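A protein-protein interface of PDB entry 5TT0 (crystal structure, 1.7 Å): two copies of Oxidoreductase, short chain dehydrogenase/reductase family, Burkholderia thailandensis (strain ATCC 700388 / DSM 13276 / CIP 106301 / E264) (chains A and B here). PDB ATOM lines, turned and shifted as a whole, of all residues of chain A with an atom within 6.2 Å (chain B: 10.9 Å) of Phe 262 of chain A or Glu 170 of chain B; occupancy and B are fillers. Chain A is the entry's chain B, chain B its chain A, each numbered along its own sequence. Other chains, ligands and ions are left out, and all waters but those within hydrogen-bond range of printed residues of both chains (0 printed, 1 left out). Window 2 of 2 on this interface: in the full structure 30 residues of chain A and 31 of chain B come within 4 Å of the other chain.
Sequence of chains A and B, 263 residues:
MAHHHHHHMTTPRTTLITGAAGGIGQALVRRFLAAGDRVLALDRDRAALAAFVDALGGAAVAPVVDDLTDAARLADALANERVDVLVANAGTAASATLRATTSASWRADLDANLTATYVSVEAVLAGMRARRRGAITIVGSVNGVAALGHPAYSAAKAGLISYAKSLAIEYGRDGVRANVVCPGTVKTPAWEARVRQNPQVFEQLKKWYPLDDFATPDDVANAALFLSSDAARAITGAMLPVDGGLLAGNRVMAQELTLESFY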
ATOM      1  N   PRO A 210     -19.898   1.808 -31.158  1.00  0.00           N
ATOM      2  CA  PRO A 210     -18.981   0.705 -30.824  1.00  0.00           C
ATOM      3  C   PRO A 210     -19.144  -0.519 -31.707  1.00  0.00           C
ATOM      4  O   PRO A 210     -18.139  -1.128 -32.102  1.00  0.00           O
ATOM      5  CB  PRO A 210     -19.336   0.410 -29.362  1.00  0.00           C
ATOM      6  CG  PRO A 210     -19.687   1.790 -28.813  1.00  0.00           C
ATOM      7  CD  PRO A 210     -20.488   2.421 -29.953  1.00  0.00           C
ATOM      8  N   ASP A 212     -19.766  -0.554 -34.677  1.00  0.00           N
ATOM      9  CA  ASP A 212     -19.279  -0.181 -36.005  1.00  0.00           C
ATOM     10  C   ASP A 212     -20.336  -0.393 -37.076  1.00  0.00           C
ATOM     11  O   ASP A 212     -20.013  -0.550 -38.257  1.00  0.00           O
ATOM     12  CB  ASP A 212     -17.994  -0.944 -36.361  1.00  0.00           C
ATOM     13  CG  ASP A 212     -16.764  -0.368 -35.683  1.00  0.00           C
ATOM     14  OD1 ASP A 212     -16.367   0.765 -36.030  1.00  0.00           O
ATOM     15  OD2 ASP A 212     -16.198  -1.036 -34.796  1.00  0.00           O
ATOM     16  N   ARG A 251     -16.224   6.377 -27.786  1.00  0.00           N
ATOM     17  CA  ARG A 251     -14.988   5.684 -28.120  1.00  0.00           C
ATOM     18  C   ARG A 251     -14.050   6.543 -28.960  1.00  0.00           C
ATOM     19  O   ARG A 251     -12.841   6.283 -28.986  1.00  0.00           O
ATOM     20  CB  ARG A 251     -15.297   4.360 -28.836  1.00  0.00           C
ATOM     21  CG  ARG A 251     -15.682   4.491 -30.297  1.00  0.00           C
ATOM     22  CD  ARG A 251     -15.730   3.116 -30.975  1.00  0.00           C
ATOM     23  NE  ARG A 251     -16.231   3.215 -32.339  1.00  0.00           N
ATOM     24  CZ  ARG A 251     -16.211   2.228 -33.228  1.00  0.00           C
ATOM     25  NH1 ARG A 251     -15.692   1.039 -32.911  1.00  0.00           N
ATOM     26  NH2 ARG A 251     -16.690   2.425 -34.452  1.00  0.00           N
ATOM     27  N   VAL A 252     -14.571   7.567 -29.635  1.00  0.00           N
ATOM     28  CA  VAL A 252     -13.708   8.462 -30.398  1.00  0.00           C
ATOM     29  C   VAL A 252     -12.898   9.341 -29.453  1.00  0.00           C
ATOM     30  O   VAL A 252     -11.681   9.490 -29.605  1.00  0.00           O
ATOM     31  CB  VAL A 252     -14.546   9.298 -31.386  1.00  0.00           C
ATOM     32  CG1 VAL A 252     -13.651  10.181 -32.243  1.00  0.00           C
ATOM     33  CG2 VAL A 252     -15.368   8.369 -32.282  1.00  0.00           C
ATOM     34  N   ALA A 254     -12.370   8.516 -26.324  1.00  0.00           N
ATOM     35  CA  ALA A 254     -11.542   7.598 -25.545  1.00  0.00           C
ATOM     36  C   ALA A 254     -10.209   7.348 -26.240  1.00  0.00           C
ATOM     37  O   ALA A 254      -9.161   7.266 -25.590  1.00  0.00           O
ATOM     38  CB  ALA A 254     -12.284   6.277 -25.319  1.00  0.00           C
ATOM     39  N   GLN A 255     -10.234   7.220 -27.567  1.00  0.00           N
ATOM     40  CA  GLN A 255      -8.995   7.047 -28.321  1.00  0.00           C
ATOM     41  C   GLN A 255      -8.051   8.227 -28.102  1.00  0.00           C
ATOM     42  O   GLN A 255      -6.834   8.050 -27.964  1.00  0.00           O
ATOM     43  CB  GLN A 255      -9.324   6.868 -29.809  1.00  0.00           C
ATOM     44  CG  GLN A 255      -8.136   6.664 -30.718  1.00  0.00           C
ATOM     45  CD  GLN A 255      -8.521   6.029 -32.050  1.00  0.00           C
ATOM     46  OE1 GLN A 255      -9.300   5.064 -32.102  1.00  0.00           O
ATOM     47  NE2 GLN A 255      -7.966   6.564 -33.136  1.00  0.00           N
ATOM     48  N   THR A 258      -6.717   8.172 -24.285  1.00  0.00           N
ATOM     49  CA  THR A 258      -5.877   7.044 -23.919  1.00  0.00           C
ATOM     50  C   THR A 258      -4.664   6.897 -24.820  1.00  0.00           C
ATOM     51  O   THR A 258      -3.716   6.199 -24.444  1.00  0.00           O
ATOM     52  CB  THR A 258      -6.686   5.742 -23.969  1.00  0.00           C
ATOM     53  OG1 THR A 258      -7.144   5.522 -25.309  1.00  0.00           O
ATOM     54  CG2 THR A 258      -7.894   5.823 -23.037  1.00  0.00           C
ATOM     55  N   GLU A 260      -4.680   5.226 -27.495  1.00  0.00           N
ATOM     56  CA  GLU A 260      -4.794   3.872 -28.019  1.00  0.00           C
ATOM     57  C   GLU A 260      -5.993   3.805 -28.953  1.00  0.00           C
ATOM     58  O   GLU A 260      -6.970   4.536 -28.780  1.00  0.00           O
ATOM     59  CB  GLU A 260      -4.968   2.829 -26.894  1.00  0.00           C
ATOM     60  CG  GLU A 260      -3.739   2.625 -26.012  1.00  0.00           C
ATOM     61  CD  GLU A 260      -3.798   1.320 -25.230  1.00  0.00           C
ATOM     62  OE1 GLU A 260      -4.485   0.383 -25.689  1.00  0.00           O
ATOM     63  OE2 GLU A 260      -3.164   1.232 -24.156  1.00  0.00           O
ATOM     64  N   SER A 261      -5.922   2.906 -29.929  1.00  0.00           N
ATOM     65  CA  SER A 261      -6.972   2.794 -30.935  1.00  0.00           C
ATOM     66  C   SER A 261      -8.196   2.073 -30.374  1.00  0.00           C
ATOM     67  O   SER A 261      -8.070   1.041 -29.709  1.00  0.00           O
ATOM     68  CB  SER A 261      -6.439   2.061 -32.165  1.00  0.00           C
ATOM     69  OG  SER A 261      -7.423   1.967 -33.179  1.00  0.00           O
ATOM     70  N   PHE A 262      -9.384   2.633 -30.630  1.00  0.00           N
ATOM     71  CA  PHE A 262     -10.647   1.992 -30.278  1.00  0.00           C
ATOM     72  C   PHE A 262     -11.472   1.572 -31.485  1.00  0.00           C
ATOM     73  O   PHE A 262     -12.512   0.928 -31.309  1.00  0.00           O
ATOM     74  CB  PHE A 262     -11.497   2.920 -29.394  1.00  0.00           C
ATOM     75  CG  PHE A 262     -11.134   2.870 -27.938  1.00  0.00           C
ATOM     76  CD1 PHE A 262     -12.024   2.374 -27.005  1.00  0.00           C
ATOM     77  CD2 PHE A 262      -9.898   3.321 -27.505  1.00  0.00           C
ATOM     78  CE1 PHE A 262     -11.688   2.326 -25.650  1.00  0.00           C
ATOM     79  CE2 PHE A 262      -9.552   3.277 -26.164  1.00  0.00           C
ATOM     80  CZ  PHE A 262     -10.449   2.771 -25.234  1.00  0.00           C
ATOM     81  N   TYR A 263     -11.047   1.919 -32.696  1.00  0.00           N
ATOM     82  CA  TYR A 263     -11.787   1.564 -33.904  1.00  0.00           C
ATOM     83  C   TYR A 263     -10.893   1.603 -35.138  1.00  0.00           C
ATOM     84  O   TYR A 263      -9.980   2.422 -35.235  1.00  0.00           O
ATOM     85  CB  TYR A 263     -12.985   2.499 -34.096  1.00  0.00           C
ATOM     86  CG  TYR A 263     -12.636   3.968 -34.175  1.00  0.00           C
ATOM     87  CD1 TYR A 263     -12.496   4.606 -35.402  1.00  0.00           C
ATOM     88  CD2 TYR A 263     -12.458   4.723 -33.021  1.00  0.00           C
ATOM     89  CE1 TYR A 263     -12.183   5.954 -35.477  1.00  0.00           C
ATOM     90  CE2 TYR A 263     -12.140   6.071 -33.088  1.00  0.00           C
ATOM     91  CZ  TYR A 263     -12.006   6.680 -34.317  1.00  0.00           C
ATOM     92  OH  TYR A 263     -11.693   8.018 -34.381  1.00  0.00           O
ATOM     93  OXT TYR A 263     -11.067   0.814 -36.068  1.00  0.00           O
ATOM     94  N   TYR B 118     -14.397  -9.459 -13.724  1.00  0.00           N
ATOM     95  CA  TYR B 118     -13.227  -9.191 -14.553  1.00  0.00           C
ATOM     96  C   TYR B 118     -12.480 -10.483 -14.873  1.00  0.00           C
ATOM     97  O   TYR B 118     -12.122 -10.751 -16.028  1.00  0.00           O
ATOM     98  CB  TYR B 118     -12.307  -8.186 -13.837  1.00  0.00           C
ATOM     99  CG  TYR B 118     -11.018  -7.938 -14.575  1.00  0.00           C
ATOM    100  CD1 TYR B 118     -10.937  -6.947 -15.550  1.00  0.00           C
ATOM    101  CD2 TYR B 118      -9.883  -8.701 -14.317  1.00  0.00           C
ATOM    102  CE1 TYR B 118      -9.760  -6.724 -16.240  1.00  0.00           C
ATOM    103  CE2 TYR B 118      -8.700  -8.484 -15.008  1.00  0.00           C
ATOM    104  CZ  TYR B 118      -8.647  -7.494 -15.966  1.00  0.00           C
ATOM    105  OH  TYR B 118      -7.483  -7.280 -16.659  1.00  0.00           O
ATOM    106  N   VAL B 121     -14.438 -12.617 -17.391  1.00  0.00           N
ATOM    107  CA  VAL B 121     -14.346 -12.073 -18.750  1.00  0.00           C
ATOM    108  C   VAL B 121     -12.984 -12.381 -19.359  1.00  0.00           C
ATOM    109  O   VAL B 121     -12.881 -12.848 -20.501  1.00  0.00           O
ATOM    110  CB  VAL B 121     -14.605 -10.555 -18.743  1.00  0.00           C
ATOM    111  CG1 VAL B 121     -14.201  -9.951 -20.079  1.00  0.00           C
ATOM    112  CG2 VAL B 121     -16.068 -10.270 -18.443  1.00  0.00           C
ATOM    113  N   GLU B 122     -11.914 -12.101 -18.614  1.00  0.00           N
ATOM    114  CA  GLU B 122     -10.573 -12.293 -19.156  1.00  0.00           C
ATOM    115  C   GLU B 122     -10.294 -13.745 -19.506  1.00  0.00           C
ATOM    116  O   GLU B 122      -9.456 -14.008 -20.375  1.00  0.00           O
ATOM    117  CB  GLU B 122      -9.521 -11.786 -18.169  1.00  0.00           C
ATOM    118  CG  GLU B 122      -9.442 -10.263 -18.113  1.00  0.00           C
ATOM    119  CD  GLU B 122      -9.023  -9.654 -19.444  1.00  0.00           C
ATOM    120  OE1 GLU B 122      -7.929  -9.998 -19.938  1.00  0.00           O
ATOM    121  OE2 GLU B 122      -9.792  -8.845 -20.008  1.00  0.00           O
ATOM    122  N   LEU B 125     -12.412 -13.909 -23.154  1.00  0.00           N
ATOM    123  CA  LEU B 125     -12.526 -12.797 -24.100  1.00  0.00           C
ATOM    124  C   LEU B 125     -11.667 -12.987 -25.352  1.00  0.00           C
ATOM    125  O   LEU B 125     -12.070 -12.568 -26.443  1.00  0.00           O
ATOM    126  CB  LEU B 125     -12.160 -11.480 -23.397  1.00  0.00           C
ATOM    127  CG  LEU B 125     -12.299 -10.194 -24.213  1.00  0.00           C
ATOM    128  CD1 LEU B 125     -13.735 -10.035 -24.737  1.00  0.00           C
ATOM    129  CD2 LEU B 125     -11.906  -9.009 -23.358  1.00  0.00           C
ATOM    130  N   ARG B 129     -13.093 -12.554 -29.238  1.00  0.00           N
ATOM    131  CA  ARG B 129     -12.538 -11.580 -30.167  1.00  0.00           C
ATOM    132  C   ARG B 129     -11.951 -12.255 -31.401  1.00  0.00           C
ATOM    133  O   ARG B 129     -12.045 -11.716 -32.511  1.00  0.00           O
ATOM    134  CB  ARG B 129     -11.483 -10.744 -29.456  1.00  0.00           C
ATOM    135  CG  ARG B 129     -12.075  -9.874 -28.348  1.00  0.00           C
ATOM    136  CD  ARG B 129     -11.012  -9.042 -27.657  1.00  0.00           C
ATOM    137  NE  ARG B 129     -10.271  -8.223 -28.608  1.00  0.00           N
ATOM    138  CZ  ARG B 129      -8.958  -8.290 -28.776  1.00  0.00           C
ATOM    139  NH1 ARG B 129      -8.246  -9.134 -28.044  1.00  0.00           N
ATOM    140  NH2 ARG B 129      -8.357  -7.512 -29.666  1.00  0.00           N
ATOM    141  N   ILE B 136     -21.273 -10.843 -23.470  1.00  0.00           N
ATOM    142  CA  ILE B 136     -21.012 -10.824 -22.038  1.00  0.00           C
ATOM    143  C   ILE B 136     -22.238 -10.222 -21.371  1.00  0.00           C
ATOM    144  O   ILE B 136     -22.562  -9.050 -21.588  1.00  0.00           O
ATOM    145  CB  ILE B 136     -19.746 -10.022 -21.709  1.00  0.00           C
ATOM    146  CG1 ILE B 136     -18.500 -10.726 -22.268  1.00  0.00           C
ATOM    147  CG2 ILE B 136     -19.634  -9.790 -20.201  1.00  0.00           C
ATOM    148  CD1 ILE B 136     -17.320  -9.784 -22.470  1.00  0.00           C
ATOM    149  N   SER B 162     -20.268   0.289 -15.006  1.00  0.00           N
ATOM    150  CA  SER B 162     -19.139   0.966 -15.643  1.00  0.00           C
ATOM    151  C   SER B 162     -18.326  -0.003 -16.493  1.00  0.00           C
ATOM    152  O   SER B 162     -17.958   0.308 -17.633  1.00  0.00           O
ATOM    153  CB  SER B 162     -18.247   1.613 -14.568  1.00  0.00           C
ATOM    154  OG  SER B 162     -17.055   2.136 -15.138  1.00  0.00           O
ATOM    155  N   TYR B 163     -18.035  -1.187 -15.944  1.00  0.00           N
ATOM    156  CA  TYR B 163     -17.208  -2.168 -16.644  1.00  0.00           C
ATOM    157  C   TYR B 163     -17.875  -2.646 -17.931  1.00  0.00           C
ATOM    158  O   TYR B 163     -17.217  -2.780 -18.974  1.00  0.00           O
ATOM    159  CB  TYR B 163     -16.915  -3.334 -15.691  1.00  0.00           C
ATOM    160  CG  TYR B 163     -16.069  -4.460 -16.241  1.00  0.00           C
ATOM    161  CD1 TYR B 163     -14.938  -4.214 -17.029  1.00  0.00           C
ATOM    162  CD2 TYR B 163     -16.379  -5.780 -15.941  1.00  0.00           C
ATOM    163  CE1 TYR B 163     -14.164  -5.264 -17.513  1.00  0.00           C
ATOM    164  CE2 TYR B 163     -15.611  -6.840 -16.423  1.00  0.00           C
ATOM    165  CZ  TYR B 163     -14.506  -6.567 -17.209  1.00  0.00           C
ATOM    166  OH  TYR B 163     -13.744  -7.604 -17.684  1.00  0.00           O
ATOM    167  N   ALA B 164     -19.176  -2.911 -17.874  1.00  0.00           N
ATOM    168  CA  ALA B 164     -19.903  -3.279 -19.080  1.00  0.00           C
ATOM    169  C   ALA B 164     -19.765  -2.212 -20.154  1.00  0.00           C
ATOM    170  O   ALA B 164     -19.580  -2.534 -21.330  1.00  0.00           O
ATOM    171  CB  ALA B 164     -21.377  -3.508 -18.757  1.00  0.00           C
ATOM    172  N   LYS B 165     -19.861  -0.931 -19.774  1.00  0.00           N
ATOM    173  CA  LYS B 165     -19.751   0.132 -20.770  1.00  0.00           C
ATOM    174  C   LYS B 165     -18.335   0.227 -21.310  1.00  0.00           C
ATOM    175  O   LYS B 165     -18.139   0.476 -22.510  1.00  0.00           O
ATOM    176  CB  LYS B 165     -20.193   1.472 -20.171  1.00  0.00           C
ATOM    177  CG  LYS B 165     -21.693   1.514 -19.825  1.00  0.00           C
ATOM    178  CD  LYS B 165     -22.007   2.892 -19.265  1.00  0.00           C
ATOM    179  CE  LYS B 165     -23.379   3.009 -18.675  1.00  0.00           C
ATOM    180  NZ  LYS B 165     -23.452   4.333 -17.984  1.00  0.00           N
ATOM    181  N   SER B 166     -17.331   0.034 -20.442  1.00  0.00           N
ATOM    182  CA  SER B 166     -15.947   0.012 -20.906  1.00  0.00           C
ATOM    183  C   SER B 166     -15.713  -1.145 -21.874  1.00  0.00           C
ATOM    184  O   SER B 166     -15.066  -0.970 -22.918  1.00  0.00           O
ATOM    185  CB  SER B 166     -14.991  -0.071 -19.711  1.00  0.00           C
ATOM    186  OG  SER B 166     -14.992   1.150 -18.966  1.00  0.00           O
ATOM    187  N   LEU B 167     -16.226  -2.331 -21.543  1.00  0.00           N
ATOM    188  CA  LEU B 167     -16.154  -3.454 -22.476  1.00  0.00           C
ATOM    189  C   LEU B 167     -16.840  -3.111 -23.790  1.00  0.00           C
ATOM    190  O   LEU B 167     -16.321  -3.411 -24.872  1.00  0.00           O
ATOM    191  CB  LEU B 167     -16.812  -4.689 -21.861  1.00  0.00           C
ATOM    192  CG  LEU B 167     -16.071  -5.393 -20.718  1.00  0.00           C
ATOM    193  CD1 LEU B 167     -17.023  -6.331 -19.980  1.00  0.00           C
ATOM    194  CD2 LEU B 167     -14.889  -6.185 -21.264  1.00  0.00           C
ATOM    195  N   ALA B 168     -18.012  -2.489 -23.712  1.00  0.00           N
ATOM    196  CA  ALA B 168     -18.779  -2.229 -24.925  1.00  0.00           C
ATOM    197  C   ALA B 168     -18.006  -1.328 -25.888  1.00  0.00           C
ATOM    198  O   ALA B 168     -17.933  -1.612 -27.088  1.00  0.00           O
ATOM    199  CB  ALA B 168     -20.138  -1.621 -24.570  1.00  0.00           C
ATOM    200  N   ILE B 169     -17.403  -0.240 -25.384  1.00  0.00           N
ATOM    201  CA  ILE B 169     -16.784   0.691 -26.329  1.00  0.00           C
ATOM    202  C   ILE B 169     -15.450   0.170 -26.847  1.00  0.00           C
ATOM    203  O   ILE B 169     -15.021   0.544 -27.947  1.00  0.00           O
ATOM    204  CB  ILE B 169     -16.624   2.107 -25.727  1.00  0.00           C
ATOM    205  CG1 ILE B 169     -15.586   2.147 -24.596  1.00  0.00           C
ATOM    206  CG2 ILE B 169     -17.966   2.660 -25.280  1.00  0.00           C
ATOM    207  CD1 ILE B 169     -15.025   3.576 -24.333  1.00  0.00           C
ATOM    208  N   GLU B 170     -14.767  -0.685 -26.087  1.00  0.00           N
ATOM    209  CA  GLU B 170     -13.440  -1.118 -26.495  1.00  0.00           C
ATOM    210  C   GLU B 170     -13.470  -2.346 -27.396  1.00  0.00           C
ATOM    211  O   GLU B 170     -12.613  -2.477 -28.283  1.00  0.00           O
ATOM    212  CB  GLU B 170     -12.572  -1.396 -25.262  1.00  0.00           C
ATOM    213  CG  GLU B 170     -11.117  -1.703 -25.602  1.00  0.00           C
ATOM    214  CD  GLU B 170     -10.178  -1.583 -24.408  1.00  0.00           C
ATOM    215  OE1 GLU B 170      -9.039  -2.098 -24.504  1.00  0.00           O
ATOM    216  OE2 GLU B 170     -10.572  -0.959 -23.394  1.00  0.00           O
ATOM    217  N   TYR B 171     -14.450  -3.230 -27.212  1.00  0.00           N
ATOM    218  CA  TYR B 171     -14.454  -4.500 -27.916  1.00  0.00           C
ATOM    219  C   TYR B 171     -15.631  -4.666 -28.863  1.00  0.00           C
ATOM    220  O   TYR B 171     -15.748  -5.721 -29.500  1.00  0.00           O
ATOM    221  CB  TYR B 171     -14.419  -5.650 -26.903  1.00  0.00           C
ATOM    222  CG  TYR B 171     -13.132  -5.656 -26.115  1.00  0.00           C
ATOM    223  CD1 TYR B 171     -11.912  -5.833 -26.758  1.00  0.00           C
ATOM    224  CD2 TYR B 171     -13.126  -5.452 -24.737  1.00  0.00           C
ATOM    225  CE1 TYR B 171     -10.726  -5.829 -26.053  1.00  0.00           C
ATOM    226  CE2 TYR B 171     -11.939  -5.446 -24.022  1.00  0.00           C
ATOM    227  CZ  TYR B 171     -10.746  -5.636 -24.686  1.00  0.00           C
ATOM    228  OH  TYR B 171      -9.560  -5.643 -23.986  1.00  0.00           O
ATOM    229  N   GLY B 172     -16.490  -3.657 -28.991  1.00  0.00           N
ATOM    230  CA  GLY B 172     -17.534  -3.715 -29.997  1.00  0.00           C
ATOM    231  C   GLY B 172     -16.985  -3.878 -31.399  1.00  0.00           C
ATOM    232  O   GLY B 172     -17.576  -4.583 -32.222  1.00  0.00           O
ATOM    233  N   ARG B 173     -15.831  -3.259 -31.681  1.00  0.00           N
ATOM    234  CA  ARG B 173     -15.177  -3.426 -32.974  1.00  0.00           C
ATOM    235  C   ARG B 173     -14.778  -4.870 -33.242  1.00  0.00           C
ATOM    236  O   ARG B 173     -14.477  -5.216 -34.390  1.00  0.00           O
ATOM    237  CB  ARG B 173     -13.939  -2.529 -33.047  1.00  0.00           C
ATOM    238  N   ASP B 174     -14.730  -5.704 -32.203  1.00  0.00           N
ATOM    239  CA  ASP B 174     -14.421  -7.122 -32.323  1.00  0.00           C
ATOM    240  C   ASP B 174     -15.677  -7.983 -32.308  1.00  0.00           C
ATOM    241  O   ASP B 174     -15.577  -9.208 -32.165  1.00  0.00           O
ATOM    242  CB  ASP B 174     -13.478  -7.560 -31.194  1.00  0.00           C
ATOM    243  CG  ASP B 174     -12.109  -6.902 -31.279  1.00  0.00           C
ATOM    244  OD1 ASP B 174     -11.607  -6.724 -32.414  1.00  0.00           O
ATOM    245  OD2 ASP B 174     -11.541  -6.556 -30.219  1.00  0.00           O
ATOM    246  N   GLY B 175     -16.853  -7.374 -32.427  1.00  0.00           N
ATOM    247  CA  GLY B 175     -18.079  -8.146 -32.390  1.00  0.00           C
ATOM    248  C   GLY B 175     -18.454  -8.692 -31.030  1.00  0.00           C
ATOM    249  O   GLY B 175     -19.211  -9.664 -30.955  1.00  0.00           O
ATOM    250  N   VAL B 176     -17.941  -8.104 -29.948  1.00  0.00           N
ATOM    251  CA  VAL B 176     -18.269  -8.522 -28.590  1.00  0.00           C
ATOM    252  C   VAL B 176     -19.193  -7.485 -27.969  1.00  0.00           C
ATOM    253  O   VAL B 176     -18.875  -6.289 -27.961  1.00  0.00           O
ATOM    254  CB  VAL B 176     -17.014  -8.697 -27.725  1.00  0.00           C
ATOM    255  CG1 VAL B 176     -17.426  -9.119 -26.310  1.00  0.00           C
ATOM    256  CG2 VAL B 176     -16.072  -9.716 -28.349  1.00  0.00           C
ATOM    257  N   ARG B 177     -20.317  -7.949 -27.423  1.00  0.00           N
ATOM    258  CA  ARG B 177     -21.283  -7.104 -26.743  1.00  0.00           C
ATOM    259  C   ARG B 177     -21.219  -7.346 -25.240  1.00  0.00           C
ATOM    260  O   ARG B 177     -20.870  -8.440 -24.792  1.00  0.00           O
ATOM    261  CB  ARG B 177     -22.699  -7.398 -27.249  1.00  0.00           C
ATOM    262  CG  ARG B 177     -22.864  -7.127 -28.733  1.00  0.00           C
ATOM    263  CD  ARG B 177     -24.322  -7.227 -29.155  1.00  0.00           C
ATOM    264  NE  ARG B 177     -24.811  -8.587 -29.028  1.00  0.00           N
ATOM    265  CZ  ARG B 177     -25.616  -9.013 -28.055  1.00  0.00           C
ATOM    266  NH1 ARG B 177     -26.037  -8.180 -27.116  1.00  0.00           N
ATOM    267  NH2 ARG B 177     -25.992 -10.285 -28.030  1.00  0.00           N
ATOM    268  N   ALA B 178     -21.550  -6.320 -24.463  1.00  0.00           N
ATOM    269  CA  ALA B 178     -21.523  -6.439 -23.009  1.00  0.00           C
ATOM    270  C   ALA B 178     -22.675  -5.648 -22.418  1.00  0.00           C
ATOM    271  O   ALA B 178     -22.816  -4.461 -22.708  1.00  0.00           O
ATOM    272  CB  ALA B 178     -20.192  -5.939 -22.430  1.00  0.00           C
ATOM    273  N   THR B 236     -25.648  -3.037 -26.718  1.00  0.00           N
ATOM    274  CA  THR B 236     -24.430  -3.221 -25.950  1.00  0.00           C
ATOM    275  C   THR B 236     -24.215  -1.985 -25.083  1.00  0.00           C
ATOM    276  O   THR B 236     -24.555  -0.867 -25.480  1.00  0.00           O
ATOM    277  CB  THR B 236     -23.218  -3.494 -26.862  1.00  0.00           C
ATOM    278  OG1 THR B 236     -22.089  -3.873 -26.072  1.00  0.00           O
ATOM    279  CG2 THR B 236     -22.858  -2.275 -27.693  1.00  0.00           C
ATOM    280  N   GLY B 237     -23.676  -2.210 -23.889  1.00  0.00           N
ATOM    281  CA  GLY B 237     -23.533  -1.137 -22.923  1.00  0.00           C
ATOM    282  C   GLY B 237     -24.808  -0.814 -22.175  1.00  0.00           C
ATOM    283  O   GLY B 237     -24.875   0.227 -21.500  1.00  0.00           O
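Among the printed residues, merely in contact across the chains: Pro 210 of chain A with Ala 168 of chain B (3.4 Å), Pro 210 of chain A with Ile 169 of chain B (3.97 Å), Pro 210 of chain A with Gly 172 of chain B (3.1 Å), Asp 212 of chain A with Arg 173 of chain B (3.2 Å), Arg 251 of chain A with Ile 169 of chain B (3.9 Å), Arg 251 of chain A with Arg 173 of chain B (3.98 Å), Ala 254 of chain A with Ile 169 of chain B (3.97 Å), Phe 262 of chain A with Ile 169 of chain B (3.6 Å) and Phe 262 of chain A with Glu 170 of chain B (3.8 Å).
NH1 of Arg 251 of chain A sits at hydrogen-bond distance from O of Pro 210 of chain A, at 3.4 Å.
NH1 of Arg 251 of chain A is in salt-bridge range of OD2 of Asp 212 of chain A (2.8 Å).
The backbone carbonyl oxygen (O) of Ala 254 of chain A sits at hydrogen-bond distance from the side-chain hydroxyl (OG1) of Thr 258 of chain A (2.7 Å).
The side-chain amide oxygen of Gln 255 of chain A lies within hydrogen-bond range of the backbone NH of Phe 262 of chain A (2.8 Å).
N of Arg 173 of chain B is in hydrogen-bond range of O of Pro 210 of chain A (3.2 Å).
Printed residues of chain B that touch a printed residue of chain A: Ala 168, Ile 169, Glu 170, Gly 172 and Arg 173.
Along chain B the printed residues that touch a printed residue of chain A span positions 168 to 173.
Of the 11 printed residues of chain A, 5 touch a printed residue of chain B.
Printed residues of chain A that touch a printed residue of chain B: Pro 210, Asp 212, Arg 251, Ala 254 and Phe 262.
Hydrophobic or aromatic side chains of chain A that line the printed part of chain B: Pro 210, Ala 254 and Phe 262.
Among the printed residues, no Asp or Glu carboxylate lies within 4 Å of a Lys or Arg side-chain nitrogen of the other chain.
No position is printed for both chains.
Of the 10 pairs that touch across the chains among the printed residues, none has its exchanged pair printed and touching as well.
Of chain B, only Ile 169 and Glu 170 come within 4 Å of Phe 262 of chain A.
Glu 170 of chain B touches just one residue of chain A: Phe 262 (3.8 Å).
Ala 254 of chain A touches just one residue of chain B: Ile 169 (3.97 Å).
No residue of chain B comes within 4 Å of Gln 255 of chain A.
No residue of chain B comes within 4 Å of Thr 258 of chain A.
No residue of chain B comes within 4 Å of Ser 261 of chain A.
Of the printed residues of chain A, Arg 173 of chain B touches Pro 210, Asp 212 and Arg 251.
Of the printed residues of chain A, Ile 169 of chain B touches Pro 210 (3.97 Å), Arg 251 (3.9 Å), Ala 254 (3.97 Å) and Phe 262 (3.6 Å).
Of the printed residues of chain B, Asp 212 of chain A touches Arg 173.
Of the printed residues of chain A, Ala 168 of chain B touches Pro 210.
Printed residues of chain B within 4 Å of Pro 210 of chain A: Ala 168, Ile 169, Gly 172 and Arg 173.
Tyr 118 of chain B touches none of the printed residues of chain A.
The nearest residue of chain B that does not touch Phe 262 of chain A is Arg 173 of chain B (4.1 Å).
The nearest residue of chain A that does not touch Glu 170 of chain B is Glu 260 of chain A (5.3 Å).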
